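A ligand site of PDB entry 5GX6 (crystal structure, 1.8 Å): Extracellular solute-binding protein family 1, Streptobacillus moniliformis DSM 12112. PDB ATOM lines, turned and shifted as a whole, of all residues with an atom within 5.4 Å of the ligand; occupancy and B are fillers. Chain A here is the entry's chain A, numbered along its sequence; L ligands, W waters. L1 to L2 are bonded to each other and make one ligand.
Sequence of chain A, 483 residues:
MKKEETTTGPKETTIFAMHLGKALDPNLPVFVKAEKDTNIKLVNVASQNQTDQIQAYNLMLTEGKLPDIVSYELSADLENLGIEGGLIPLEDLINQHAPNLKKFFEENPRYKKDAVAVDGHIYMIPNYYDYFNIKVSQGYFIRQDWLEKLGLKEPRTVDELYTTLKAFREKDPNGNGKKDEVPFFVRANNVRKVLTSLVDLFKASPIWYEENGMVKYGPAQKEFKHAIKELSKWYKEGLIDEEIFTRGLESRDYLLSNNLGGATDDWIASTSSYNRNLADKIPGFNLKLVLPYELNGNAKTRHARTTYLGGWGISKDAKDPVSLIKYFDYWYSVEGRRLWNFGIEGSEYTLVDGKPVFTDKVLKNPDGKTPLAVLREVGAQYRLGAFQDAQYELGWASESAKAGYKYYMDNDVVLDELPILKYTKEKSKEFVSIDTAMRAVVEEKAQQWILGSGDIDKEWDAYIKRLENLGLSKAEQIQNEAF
Water W1 bridges O5 of LIG L1 (2.6 Å) and O of Arg 187 (2.7 Å).
Water W2 lies within hydrogen-bond range of an oxygen (O5) of LIG L1 (2.7 Å) and the indole nitrogen of Trp 267 (2.9 Å).
Water W7 lies within hydrogen-bond range of the side-chain amide oxygen (OE1) of Gln 381, an oxygen (O1) of LG2 L2, the guanidinium group (NH2) of Arg 376 and the side-chain amide nitrogen (NE2) of Gln 388.
Water W8 lies within hydrogen-bond range of the side-chain carboxylate of Glu 73 (2.6 Å), an oxygen (O1) of LIG L1 (2.8 Å) and the side-chain amino group of Lys 193 (2.9 Å).
Water W3 lies within hydrogen-bond range of O5 of LG2 L2 (2.8 Å), OE1 of Glu 393 (2.9 Å) and N of Ala 269 (3.0 Å).
Water W4 lies within hydrogen-bond range of O of Gln 381 (2.8 Å), O6 of LIG L1 (3.0 Å), N of Arg 383 (3.3 Å) and ND2 of Asn 127 (3.3 Å).
The guanidinium group (NH1) of Arg 252 is in hydrogen-bond range of the side-chain hydroxyl (OG) of Ser 270 (2.9 Å).
The side-chain carboxylate (OE2) of Glu 393 lies within salt-bridge range of the guanidinium group (NH1) of Arg 305, 3.0 Å away.
NH1 of Arg 376 is in hydrogen-bond range of O of Gln 381.
The side-chain amide oxygen of Gln 388 lies within hydrogen-bond range of the guanidinium group of Arg 305 (3.4 Å).
O of Tyr 392 lies close to NE1 of Trp 396, at 3.3 Å.
O of Trp 267 lies within hydrogen-bond range of OG1 of Thr 271.
N of Leu 309 sits at hydrogen-bond distance from O of Asn 127 (2.9 Å).
The backbone carbonyl oxygen (O) of Trp 340 is in hydrogen-bond range of the backbone NH (N) of Gln 381 (2.9 Å).
The backbone NH of Ser 270 sits at hydrogen-bond distance from an oxygen (O5) of LG2 L2, at 3.0 Å.
O4 of LG2 L2 is in hydrogen-bond range of OG of Ser 270 (2.6 Å).
An oxygen (O2) of LG2 L2 sits at hydrogen-bond distance from the side-chain carboxylate of Glu 393 (2.7 Å).
NE of Arg 376 lies within salt-bridge range of O7 of LIG L1, at 2.7 Å.
NZ of Lys 193 is in hydrogen-bond range of O5 of LIG L1 (2.8 Å).
NH2 of Arg 187 is in salt-bridge range of O8 of LIG L1, at 2.8 Å.
The side-chain amide nitrogen of Gln 388 sits at hydrogen-bond distance from an oxygen (O1) of LG2 L2, at 2.9 Å.
A ring nitrogen (NE2) of His 19 sits at hydrogen-bond distance from an oxygen (O6) of LIG L1.
OH of Tyr 392 sits at hydrogen-bond distance from O2 of LG2 L2 (2.9 Å).
The side-chain hydroxyl (OH) of Tyr 129 lies within hydrogen-bond range of a nitrogen (N1) of LIG L1, at 2.9 Å.
CD1 of Leu 20 touches O9 of LIG L1 (3.4 Å).
CB of Trp 267 touches O4 of LG2 L2 (3.1 Å).
CB of Ala 269 touches O5 of LG2 L2, 3.6 Å away.
NH1 of Arg 305 touches O2 of LG2 L2, 3.7 Å away.
CD2 of Leu 309 touches O1 of LIG L1 (3.4 Å).
Leu 372 touches the ligand.
O of Gln 381 touches O6 of LIG L1, at 3.8 Å.
CH2 of Trp 396 touches O5 of LG2 L2 (3.8 Å).
Hydrophobic or aromatic side chains that line the ligand: His 19, Leu 20, Tyr 129, Trp 267, Ala 269, Leu 309, Leu 372, Tyr 392 and Trp 396.
Within 4 Å of the ligand: His 19, Leu 20, Tyr 129, Arg 187, Lys 193, Trp 267, Ala 269, Ser 270, Arg 305, Leu 309, Leu 372, Arg 376, Gln 381, Gln 388, Tyr 392, Glu 393 and Trp 396.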
ATOM      1  N   HIS A  19      17.168  32.436 -30.024  1.00  0.00           N
ATOM      2  CA  HIS A  19      17.469  31.371 -29.076  1.00  0.00           C
ATOM      3  C   HIS A  19      17.722  30.086 -29.851  1.00  0.00           C
ATOM      4  O   HIS A  19      16.935  29.723 -30.722  1.00  0.00           O
ATOM      5  CB  HIS A  19      16.332  31.160 -28.082  1.00  0.00           C
ATOM      6  CG  HIS A  19      16.634  30.152 -27.022  1.00  0.00           C
ATOM      7  ND1 HIS A  19      17.818  30.164 -26.311  1.00  0.00           N
ATOM      8  CD2 HIS A  19      15.933  29.079 -26.576  1.00  0.00           C
ATOM      9  CE1 HIS A  19      17.831  29.153 -25.461  1.00  0.00           C
ATOM     10  NE2 HIS A  19      16.701  28.490 -25.596  1.00  0.00           N
ATOM     11  N   LEU A  20      18.799  29.390 -29.495  1.00  0.00           N
ATOM     12  CA  LEU A  20      19.164  28.119 -30.136  1.00  0.00           C
ATOM     13  C   LEU A  20      19.189  28.270 -31.653  1.00  0.00           C
ATOM     14  O   LEU A  20      18.697  27.417 -32.391  1.00  0.00           O
ATOM     15  CB  LEU A  20      18.219  27.002 -29.686  1.00  0.00           C
ATOM     16  CG  LEU A  20      18.338  26.656 -28.198  1.00  0.00           C
ATOM     17  CD1 LEU A  20      17.197  25.752 -27.737  1.00  0.00           C
ATOM     18  CD2 LEU A  20      19.679  25.971 -27.946  1.00  0.00           C
ATOM     19  N   GLU A  73      21.497  36.289 -24.721  1.00  0.00           N
ATOM     20  CA  GLU A  73      21.954  35.203 -23.878  1.00  0.00           C
ATOM     21  C   GLU A  73      23.134  35.579 -22.999  1.00  0.00           C
ATOM     22  O   GLU A  73      23.331  34.963 -21.944  1.00  0.00           O
ATOM     23  CB  GLU A  73      22.317  33.972 -24.722  1.00  0.00           C
ATOM     24  CG  GLU A  73      22.625  32.714 -23.878  1.00  0.00           C
ATOM     25  CD  GLU A  73      22.679  31.424 -24.672  1.00  0.00           C
ATOM     26  OE1 GLU A  73      21.763  31.161 -25.488  1.00  0.00           O
ATOM     27  OE2 GLU A  73      23.639  30.653 -24.479  1.00  0.00           O
ATOM     28  N   ASN A 127      16.312  34.958 -17.483  1.00  0.00           N
ATOM     29  CA  ASN A 127      15.534  33.754 -17.729  1.00  0.00           C
ATOM     30  C   ASN A 127      15.993  32.707 -16.718  1.00  0.00           C
ATOM     31  O   ASN A 127      17.067  32.116 -16.857  1.00  0.00           O
ATOM     32  CB  ASN A 127      15.692  33.268 -19.163  1.00  0.00           C
ATOM     33  CG  ASN A 127      14.554  32.372 -19.596  1.00  0.00           C
ATOM     34  OD1 ASN A 127      13.573  32.844 -20.159  1.00  0.00           O
ATOM     35  ND2 ASN A 127      14.666  31.072 -19.291  1.00  0.00           N
ATOM     36  N   TYR A 129      16.322  29.346 -14.565  1.00  0.00           N
ATOM     37  CA  TYR A 129      16.049  27.927 -14.396  1.00  0.00           C
ATOM     38  C   TYR A 129      15.309  27.715 -13.080  1.00  0.00           C
ATOM     39  O   TYR A 129      15.264  28.594 -12.207  1.00  0.00           O
ATOM     40  CB  TYR A 129      17.347  27.121 -14.403  1.00  0.00           C
ATOM     41  CG  TYR A 129      17.995  26.962 -15.757  1.00  0.00           C
ATOM     42  CD1 TYR A 129      17.399  26.190 -16.747  1.00  0.00           C
ATOM     43  CD2 TYR A 129      19.209  27.580 -16.062  1.00  0.00           C
ATOM     44  CE1 TYR A 129      17.987  26.028 -17.991  1.00  0.00           C
ATOM     45  CE2 TYR A 129      19.803  27.431 -17.309  1.00  0.00           C
ATOM     46  CZ  TYR A 129      19.183  26.646 -18.263  1.00  0.00           C
ATOM     47  OH  TYR A 129      19.762  26.481 -19.503  1.00  0.00           O
ATOM     48  N   ARG A 187      26.640  18.064 -29.012  1.00  0.00           N
ATOM     49  CA  ARG A 187      25.545  18.832 -29.597  1.00  0.00           C
ATOM     50  C   ARG A 187      25.754  20.306 -29.281  1.00  0.00           C
ATOM     51  O   ARG A 187      25.876  20.686 -28.118  1.00  0.00           O
ATOM     52  CB  ARG A 187      24.194  18.340 -29.075  1.00  0.00           C
ATOM     53  CG  ARG A 187      22.975  18.996 -29.730  1.00  0.00           C
ATOM     54  CD  ARG A 187      21.708  18.274 -29.261  1.00  0.00           C
ATOM     55  NE  ARG A 187      21.552  18.337 -27.814  1.00  0.00           N
ATOM     56  CZ  ARG A 187      20.803  19.228 -27.181  1.00  0.00           C
ATOM     57  NH1 ARG A 187      20.093  20.128 -27.868  1.00  0.00           N
ATOM     58  NH2 ARG A 187      20.731  19.218 -25.856  1.00  0.00           N
ATOM     59  N   LYS A 193      30.172  25.710 -27.089  1.00  0.00           N
ATOM     60  CA  LYS A 193      29.392  24.544 -26.680  1.00  0.00           C
ATOM     61  C   LYS A 193      30.049  23.236 -27.113  1.00  0.00           C
ATOM     62  O   LYS A 193      29.939  22.229 -26.402  1.00  0.00           O
ATOM     63  CB  LYS A 193      27.966  24.651 -27.198  1.00  0.00           C
ATOM     64  CG  LYS A 193      27.088  25.516 -26.306  1.00  0.00           C
ATOM     65  CD  LYS A 193      25.614  25.490 -26.740  1.00  0.00           C
ATOM     66  CE  LYS A 193      24.754  26.237 -25.721  1.00  0.00           C
ATOM     67  NZ  LYS A 193      23.312  26.290 -26.128  1.00  0.00           N
ATOM     68  N   LEU A 249      23.081  21.610 -34.182  1.00  0.00           N
ATOM     69  CA  LEU A 249      22.193  21.148 -33.124  1.00  0.00           C
ATOM     70  C   LEU A 249      21.430  19.880 -33.479  1.00  0.00           C
ATOM     71  O   LEU A 249      20.866  19.243 -32.568  1.00  0.00           O
ATOM     72  CB  LEU A 249      21.205  22.269 -32.752  1.00  0.00           C
ATOM     73  CG  LEU A 249      21.838  23.427 -32.000  1.00  0.00           C
ATOM     74  CD1 LEU A 249      20.838  24.572 -31.815  1.00  0.00           C
ATOM     75  CD2 LEU A 249      22.353  22.948 -30.651  1.00  0.00           C
ATOM     76  N   ARG A 252      22.846  15.121 -32.323  1.00  0.00           N
ATOM     77  CA  ARG A 252      22.403  13.998 -31.515  1.00  0.00           C
ATOM     78  C   ARG A 252      21.249  13.259 -32.178  1.00  0.00           C
ATOM     79  O   ARG A 252      21.237  12.029 -32.239  1.00  0.00           O
ATOM     80  CB  ARG A 252      22.005  14.500 -30.114  1.00  0.00           C
ATOM     81  CG  ARG A 252      21.461  13.434 -29.186  1.00  0.00           C
ATOM     82  CD  ARG A 252      21.012  14.059 -27.861  1.00  0.00           C
ATOM     83  NE  ARG A 252      19.949  15.044 -28.070  1.00  0.00           N
ATOM     84  CZ  ARG A 252      19.403  15.789 -27.113  1.00  0.00           C
ATOM     85  NH1 ARG A 252      19.836  15.670 -25.860  1.00  0.00           N
ATOM     86  NH2 ARG A 252      18.431  16.645 -27.402  1.00  0.00           N
ATOM     87  N   TRP A 267      22.580  17.044 -21.972  1.00  0.00           N
ATOM     88  CA  TRP A 267      21.551  17.241 -20.948  1.00  0.00           C
ATOM     89  C   TRP A 267      20.839  15.929 -20.629  1.00  0.00           C
ATOM     90  O   TRP A 267      20.512  15.150 -21.523  1.00  0.00           O
ATOM     91  CB  TRP A 267      20.558  18.288 -21.432  1.00  0.00           C
ATOM     92  CG  TRP A 267      21.114  19.670 -21.409  1.00  0.00           C
ATOM     93  CD1 TRP A 267      22.013  20.234 -22.281  1.00  0.00           C
ATOM     94  CD2 TRP A 267      20.819  20.680 -20.440  1.00  0.00           C
ATOM     95  NE1 TRP A 267      22.275  21.547 -21.913  1.00  0.00           N
ATOM     96  CE2 TRP A 267      21.561  21.834 -20.773  1.00  0.00           C
ATOM     97  CE3 TRP A 267      19.995  20.712 -19.308  1.00  0.00           C
ATOM     98  CZ2 TRP A 267      21.494  23.000 -20.027  1.00  0.00           C
ATOM     99  CZ3 TRP A 267      19.928  21.879 -18.562  1.00  0.00           C
ATOM    100  CH2 TRP A 267      20.673  23.007 -18.930  1.00  0.00           C
ATOM    101  N   ILE A 268      20.575  15.718 -19.337  1.00  0.00           N
ATOM    102  CA  ILE A 268      20.171  14.394 -18.875  1.00  0.00           C
ATOM    103  C   ILE A 268      18.769  14.040 -19.367  1.00  0.00           C
ATOM    104  O   ILE A 268      18.543  12.941 -19.893  1.00  0.00           O
ATOM    105  CB  ILE A 268      20.297  14.299 -17.348  1.00  0.00           C
ATOM    106  CG1 ILE A 268      21.774  14.163 -16.958  1.00  0.00           C
ATOM    107  CG2 ILE A 268      19.468  13.139 -16.800  1.00  0.00           C
ATOM    108  CD1 ILE A 268      22.046  14.340 -15.477  1.00  0.00           C
ATOM    109  N   ALA A 269      17.808  14.949 -19.211  1.00  0.00           N
ATOM    110  CA  ALA A 269      16.420  14.595 -19.541  1.00  0.00           C
ATOM    111  C   ALA A 269      16.243  14.365 -21.038  1.00  0.00           C
ATOM    112  O   ALA A 269      15.711  13.336 -21.460  1.00  0.00           O
ATOM    113  CB  ALA A 269      15.445  15.657 -19.029  1.00  0.00           C
ATOM    114  N   SER A 270      16.690  15.324 -21.869  1.00  0.00           N
ATOM    115  CA  SER A 270      16.469  15.175 -23.299  1.00  0.00           C
ATOM    116  C   SER A 270      17.289  14.023 -23.876  1.00  0.00           C
ATOM    117  O   SER A 270      16.841  13.363 -24.820  1.00  0.00           O
ATOM    118  CB  SER A 270      16.786  16.481 -24.031  1.00  0.00           C
ATOM    119  OG  SER A 270      18.138  16.878 -23.852  1.00  0.00           O
ATOM    120  N   THR A 271      18.492  13.775 -23.363  1.00  0.00           N
ATOM    121  CA  THR A 271      19.252  12.635 -23.863  1.00  0.00           C
ATOM    122  C   THR A 271      18.611  11.318 -23.435  1.00  0.00           C
ATOM    123  O   THR A 271      18.603  10.366 -24.212  1.00  0.00           O
ATOM    124  CB  THR A 271      20.713  12.718 -23.411  1.00  0.00           C
ATOM    125  OG1 THR A 271      21.222  14.021 -23.736  1.00  0.00           O
ATOM    126  CG2 THR A 271      21.550  11.663 -24.111  1.00  0.00           C
ATOM    127  N   ARG A 305      23.552  23.095 -13.733  1.00  0.00           N
ATOM    128  CA  ARG A 305      22.620  24.156 -14.113  1.00  0.00           C
ATOM    129  C   ARG A 305      23.007  25.432 -13.380  1.00  0.00           C
ATOM    130  O   ARG A 305      23.425  25.406 -12.221  1.00  0.00           O
ATOM    131  CB  ARG A 305      21.191  23.736 -13.800  1.00  0.00           C
ATOM    132  CG  ARG A 305      20.184  24.234 -14.801  1.00  0.00           C
ATOM    133  CD  ARG A 305      18.814  23.589 -14.629  1.00  0.00           C
ATOM    134  NE  ARG A 305      18.795  22.167 -14.978  1.00  0.00           N
ATOM    135  CZ  ARG A 305      17.767  21.569 -15.551  1.00  0.00           C
ATOM    136  NH1 ARG A 305      16.676  22.263 -15.844  1.00  0.00           N
ATOM    137  NH2 ARG A 305      17.812  20.275 -15.844  1.00  0.00           N
ATOM    138  N   LEU A 309      19.901  31.932 -17.326  1.00  0.00           N
ATOM    139  CA  LEU A 309      20.619  32.034 -18.584  1.00  0.00           C
ATOM    140  C   LEU A 309      20.053  33.214 -19.360  1.00  0.00           C
ATOM    141  O   LEU A 309      18.878  33.204 -19.715  1.00  0.00           O
ATOM    142  CB  LEU A 309      20.506  30.751 -19.415  1.00  0.00           C
ATOM    143  CG  LEU A 309      21.150  30.849 -20.793  1.00  0.00           C
ATOM    144  CD1 LEU A 309      22.666  30.754 -20.661  1.00  0.00           C
ATOM    145  CD2 LEU A 309      20.607  29.767 -21.728  1.00  0.00           C
ATOM    146  N   TRP A 340       4.430  29.650 -20.865  1.00  0.00           N
ATOM    147  CA  TRP A 340       5.826  29.595 -21.315  1.00  0.00           C
ATOM    148  C   TRP A 340       6.410  28.203 -21.133  1.00  0.00           C
ATOM    149  O   TRP A 340       7.182  27.729 -21.962  1.00  0.00           O
ATOM    150  CB  TRP A 340       6.659  30.634 -20.564  1.00  0.00           C
ATOM    151  CG  TRP A 340       8.074  30.762 -21.071  1.00  0.00           C
ATOM    152  CD1 TRP A 340       8.534  31.616 -22.021  1.00  0.00           C
ATOM    153  CD2 TRP A 340       9.212  30.007 -20.621  1.00  0.00           C
ATOM    154  NE1 TRP A 340       9.891  31.445 -22.200  1.00  0.00           N
ATOM    155  CE2 TRP A 340      10.320  30.467 -21.354  1.00  0.00           C
ATOM    156  CE3 TRP A 340       9.395  28.992 -19.680  1.00  0.00           C
ATOM    157  CZ2 TRP A 340      11.598  29.942 -21.172  1.00  0.00           C
ATOM    158  CZ3 TRP A 340      10.670  28.477 -19.496  1.00  0.00           C
ATOM    159  CH2 TRP A 340      11.755  28.952 -20.240  1.00  0.00           C
ATOM    160  N   LEU A 372      10.753  17.452 -25.811  1.00  0.00           N
ATOM    161  CA  LEU A 372      11.223  18.839 -25.721  1.00  0.00           C
ATOM    162  C   LEU A 372      11.284  19.497 -27.093  1.00  0.00           C
ATOM    163  O   LEU A 372      11.063  20.712 -27.192  1.00  0.00           O
ATOM    164  CB  LEU A 372      12.584  18.896 -25.024  1.00  0.00           C
ATOM    165  CG  LEU A 372      13.209  20.279 -24.801  1.00  0.00           C
ATOM    166  CD1 LEU A 372      12.210  21.268 -24.208  1.00  0.00           C
ATOM    167  CD2 LEU A 372      14.425  20.156 -23.902  1.00  0.00           C
ATOM    168  N   ARG A 376       9.435  23.026 -27.908  1.00  0.00           N
ATOM    169  CA  ARG A 376      10.083  24.200 -28.496  1.00  0.00           C
ATOM    170  C   ARG A 376       9.423  24.617 -29.803  1.00  0.00           C
ATOM    171  O   ARG A 376       9.380  25.814 -30.120  1.00  0.00           O
ATOM    172  CB  ARG A 376      11.574  23.957 -28.700  1.00  0.00           C
ATOM    173  CG  ARG A 376      12.359  23.863 -27.394  1.00  0.00           C
ATOM    174  CD  ARG A 376      13.859  24.067 -27.596  1.00  0.00           C
ATOM    175  NE  ARG A 376      14.565  23.912 -26.327  1.00  0.00           N
ATOM    176  CZ  ARG A 376      14.669  24.885 -25.421  1.00  0.00           C
ATOM    177  NH1 ARG A 376      14.132  26.077 -25.659  1.00  0.00           N
ATOM    178  NH2 ARG A 376      15.309  24.656 -24.286  1.00  0.00           N
ATOM    179  N   GLN A 381       9.421  27.183 -23.684  1.00  0.00           N
ATOM    180  CA  GLN A 381      10.820  27.167 -23.266  1.00  0.00           C
ATOM    181  C   GLN A 381      11.685  28.133 -24.068  1.00  0.00           C
ATOM    182  O   GLN A 381      12.916  28.021 -24.057  1.00  0.00           O
ATOM    183  CB  GLN A 381      11.414  25.755 -23.349  1.00  0.00           C
ATOM    184  CG  GLN A 381      10.704  24.757 -22.436  1.00  0.00           C
ATOM    185  CD  GLN A 381      10.831  25.135 -20.971  1.00  0.00           C
ATOM    186  OE1 GLN A 381      11.903  25.543 -20.521  1.00  0.00           O
ATOM    187  NE2 GLN A 381       9.730  25.005 -20.234  1.00  0.00           N
ATOM    188  N   ARG A 383      13.868  30.998 -24.564  1.00  0.00           N
ATOM    189  CA  ARG A 383      14.631  31.807 -23.617  1.00  0.00           C
ATOM    190  C   ARG A 383      14.370  33.289 -23.822  1.00  0.00           C
ATOM    191  O   ARG A 383      14.641  33.840 -24.896  1.00  0.00           O
ATOM    192  CB  ARG A 383      16.112  31.488 -23.758  1.00  0.00           C
ATOM    193  CG  ARG A 383      16.976  31.812 -22.543  1.00  0.00           C
ATOM    194  CD  ARG A 383      17.397  33.265 -22.496  1.00  0.00           C
ATOM    195  NE  ARG A 383      17.982  33.739 -23.756  1.00  0.00           N
ATOM    196  CZ  ARG A 383      17.888  34.998 -24.171  1.00  0.00           C
ATOM    197  NH1 ARG A 383      17.239  35.881 -23.422  1.00  0.00           N
ATOM    198  NH2 ARG A 383      18.423  35.377 -25.325  1.00  0.00           N
ATOM    199  N   GLN A 388      11.440  29.270 -15.403  1.00  0.00           N
ATOM    200  CA  GLN A 388      11.161  27.874 -15.683  1.00  0.00           C
ATOM    201  C   GLN A 388      10.505  27.187 -14.485  1.00  0.00           C
ATOM    202  O   GLN A 388      10.761  27.524 -13.324  1.00  0.00           O
ATOM    203  CB  GLN A 388      12.442  27.141 -16.076  1.00  0.00           C
ATOM    204  CG  GLN A 388      12.255  25.717 -16.540  1.00  0.00           C
ATOM    205  CD  GLN A 388      13.554  25.092 -16.978  1.00  0.00           C
ATOM    206  OE1 GLN A 388      14.376  24.680 -16.152  1.00  0.00           O
ATOM    207  NE2 GLN A 388      13.771  25.028 -18.288  1.00  0.00           N
ATOM    208  N   TYR A 392       7.374  21.149 -15.538  1.00  0.00           N
ATOM    209  CA  TYR A 392       7.327  20.908 -16.979  1.00  0.00           C
ATOM    210  C   TYR A 392       8.331  19.812 -17.348  1.00  0.00           C
ATOM    211  O   TYR A 392       7.999  18.907 -18.114  1.00  0.00           O
ATOM    212  CB  TYR A 392       7.606  22.200 -17.771  1.00  0.00           C
ATOM    213  CG  TYR A 392       8.908  22.181 -18.578  1.00  0.00           C
ATOM    214  CD1 TYR A 392      10.126  22.540 -18.000  1.00  0.00           C
ATOM    215  CD2 TYR A 392       8.915  21.747 -19.898  1.00  0.00           C
ATOM    216  CE1 TYR A 392      11.307  22.472 -18.732  1.00  0.00           C
ATOM    217  CE2 TYR A 392      10.079  21.686 -20.633  1.00  0.00           C
ATOM    218  CZ  TYR A 392      11.265  22.045 -20.050  1.00  0.00           C
ATOM    219  OH  TYR A 392      12.433  21.973 -20.786  1.00  0.00           O
ATOM    220  N   GLU A 393       9.536  19.874 -16.784  1.00  0.00           N
ATOM    221  CA  GLU A 393      10.573  18.915 -17.149  1.00  0.00           C
ATOM    222  C   GLU A 393      10.239  17.529 -16.621  1.00  0.00           C
ATOM    223  O   GLU A 393      10.344  16.527 -17.333  1.00  0.00           O
ATOM    224  CB  GLU A 393      11.929  19.389 -16.634  1.00  0.00           C
ATOM    225  CG  GLU A 393      13.130  18.598 -17.154  1.00  0.00           C
ATOM    226  CD  GLU A 393      14.452  19.289 -16.884  1.00  0.00           C
ATOM    227  OE1 GLU A 393      15.492  18.578 -16.790  1.00  0.00           O
ATOM    228  OE2 GLU A 393      14.461  20.532 -16.776  1.00  0.00           O
ATOM    229  N   TRP A 396       7.699  15.315 -18.723  1.00  0.00           N
ATOM    230  CA  TRP A 396       8.083  14.472 -19.853  1.00  0.00           C
ATOM    231  C   TRP A 396       9.349  13.663 -19.628  1.00  0.00           C
ATOM    232  O   TRP A 396       9.595  12.723 -20.392  1.00  0.00           O
ATOM    233  CB  TRP A 396       8.251  15.318 -21.135  1.00  0.00           C
ATOM    234  CG  TRP A 396       9.211  16.460 -21.018  1.00  0.00           C
ATOM    235  CD1 TRP A 396       8.912  17.746 -20.693  1.00  0.00           C
ATOM    236  CD2 TRP A 396      10.634  16.426 -21.267  1.00  0.00           C
ATOM    237  NE1 TRP A 396      10.055  18.519 -20.702  1.00  0.00           N
ATOM    238  CE2 TRP A 396      11.118  17.734 -21.048  1.00  0.00           C
ATOM    239  CE3 TRP A 396      11.538  15.427 -21.641  1.00  0.00           C
ATOM    240  CZ2 TRP A 396      12.476  18.066 -21.199  1.00  0.00           C
ATOM    241  CZ3 TRP A 396      12.887  15.755 -21.787  1.00  0.00           C
ATOM    242  CH2 TRP A 396      13.339  17.064 -21.562  1.00  0.00           C
HETATM  243  C1  LIG L   1      20.257  26.014 -23.473  1.00  0.00           C
HETATM  244  C2  LIG L   1      18.846  25.645 -23.113  1.00  0.00           C
HETATM  245  C3  LIG L   1      18.781  24.185 -22.669  1.00  0.00           C
HETATM  246  C4  LIG L   1      19.269  23.312 -23.808  1.00  0.00           C
HETATM  247  C5  LIG L   1      20.697  23.779 -24.156  1.00  0.00           C
HETATM  248  C6  LIG L   1      21.301  23.058 -25.369  1.00  0.00           C
HETATM  249  C7  LIG L   1      17.214  27.174 -22.057  1.00  0.00           C
HETATM  250  C8  LIG L   1      16.964  28.019 -20.806  1.00  0.00           C
HETATM  251  O1  LIG L   1      20.227  27.308 -24.057  1.00  0.00           O
HETATM  252  N1  LIG L   1      18.385  26.525 -22.033  1.00  0.00           N
HETATM  253  O2  LIG L   1      17.389  23.860 -22.422  1.00  0.00           O
HETATM  254  O3  LIG L   1      18.448  23.520 -24.961  1.00  0.00           O
HETATM  255  O4  LIG L   1      20.716  25.172 -24.530  1.00  0.00           O
HETATM  256  O5  LIG L   1      22.610  23.627 -25.576  1.00  0.00           O
HETATM  257  O6  LIG L   1      16.461  27.207 -23.029  1.00  0.00           O
HETATM  258  O7  LIG L   1      16.427  22.132 -25.457  1.00  0.00           O
HETATM  259  O8  LIG L   1      18.656  21.034 -25.294  1.00  0.00           O
HETATM  260  O9  LIG L   1      18.141  22.522 -27.241  1.00  0.00           O
HETATM  261  S1  LIG L   1      17.921  22.293 -25.745  1.00  0.00           S
HETATM  262  C1  LG2 L   2      17.345  22.884 -21.361  1.00  0.00           C
HETATM  263  C2  LG2 L   2      16.007  22.963 -20.671  1.00  0.00           C
HETATM  264  C3  LG2 L   2      16.007  21.979 -19.533  1.00  0.00           C
HETATM  265  C4  LG2 L   2      16.209  20.691 -20.044  1.00  0.00           C
HETATM  266  C5  LG2 L   2      16.965  20.516 -21.206  1.00  0.00           C
HETATM  267  C6  LG2 L   2      17.270  19.273 -21.738  1.00  0.00           C
HETATM  268  O1  LG2 L   2      15.813  24.286 -20.165  1.00  0.00           O
HETATM  269  O2  LG2 L   2      14.678  22.029 -18.983  1.00  0.00           O
HETATM  270  O3  LG2 L   2      17.536  21.555 -21.900  1.00  0.00           O
HETATM  271  O4  LG2 L   2      17.933  19.202 -22.796  1.00  0.00           O
HETATM  272  O5  LG2 L   2      16.920  18.213 -21.160  1.00  0.00           O
HETATM  273  O   HOH W   1      23.912  21.494 -26.452  1.00  0.00           O
HETATM  274  O   HOH W   2      24.000  23.480 -23.254  1.00  0.00           O
HETATM  275  O   HOH W   3      17.662  17.816 -18.485  1.00  0.00           O
HETATM  276  O   HOH W   4      14.454  29.137 -21.962  1.00  0.00           O
HETATM  277  O   HOH W   5      17.701  22.683 -29.835  1.00  0.00           O
HETATM  278  O   HOH W   6      16.948  29.752 -18.104  1.00  0.00           O
HETATM  279  O   HOH W   7      14.321  26.112 -21.501  1.00  0.00           O
HETATM  280  O   HOH W   8      22.841  28.196 -24.025  1.00  0.00           O
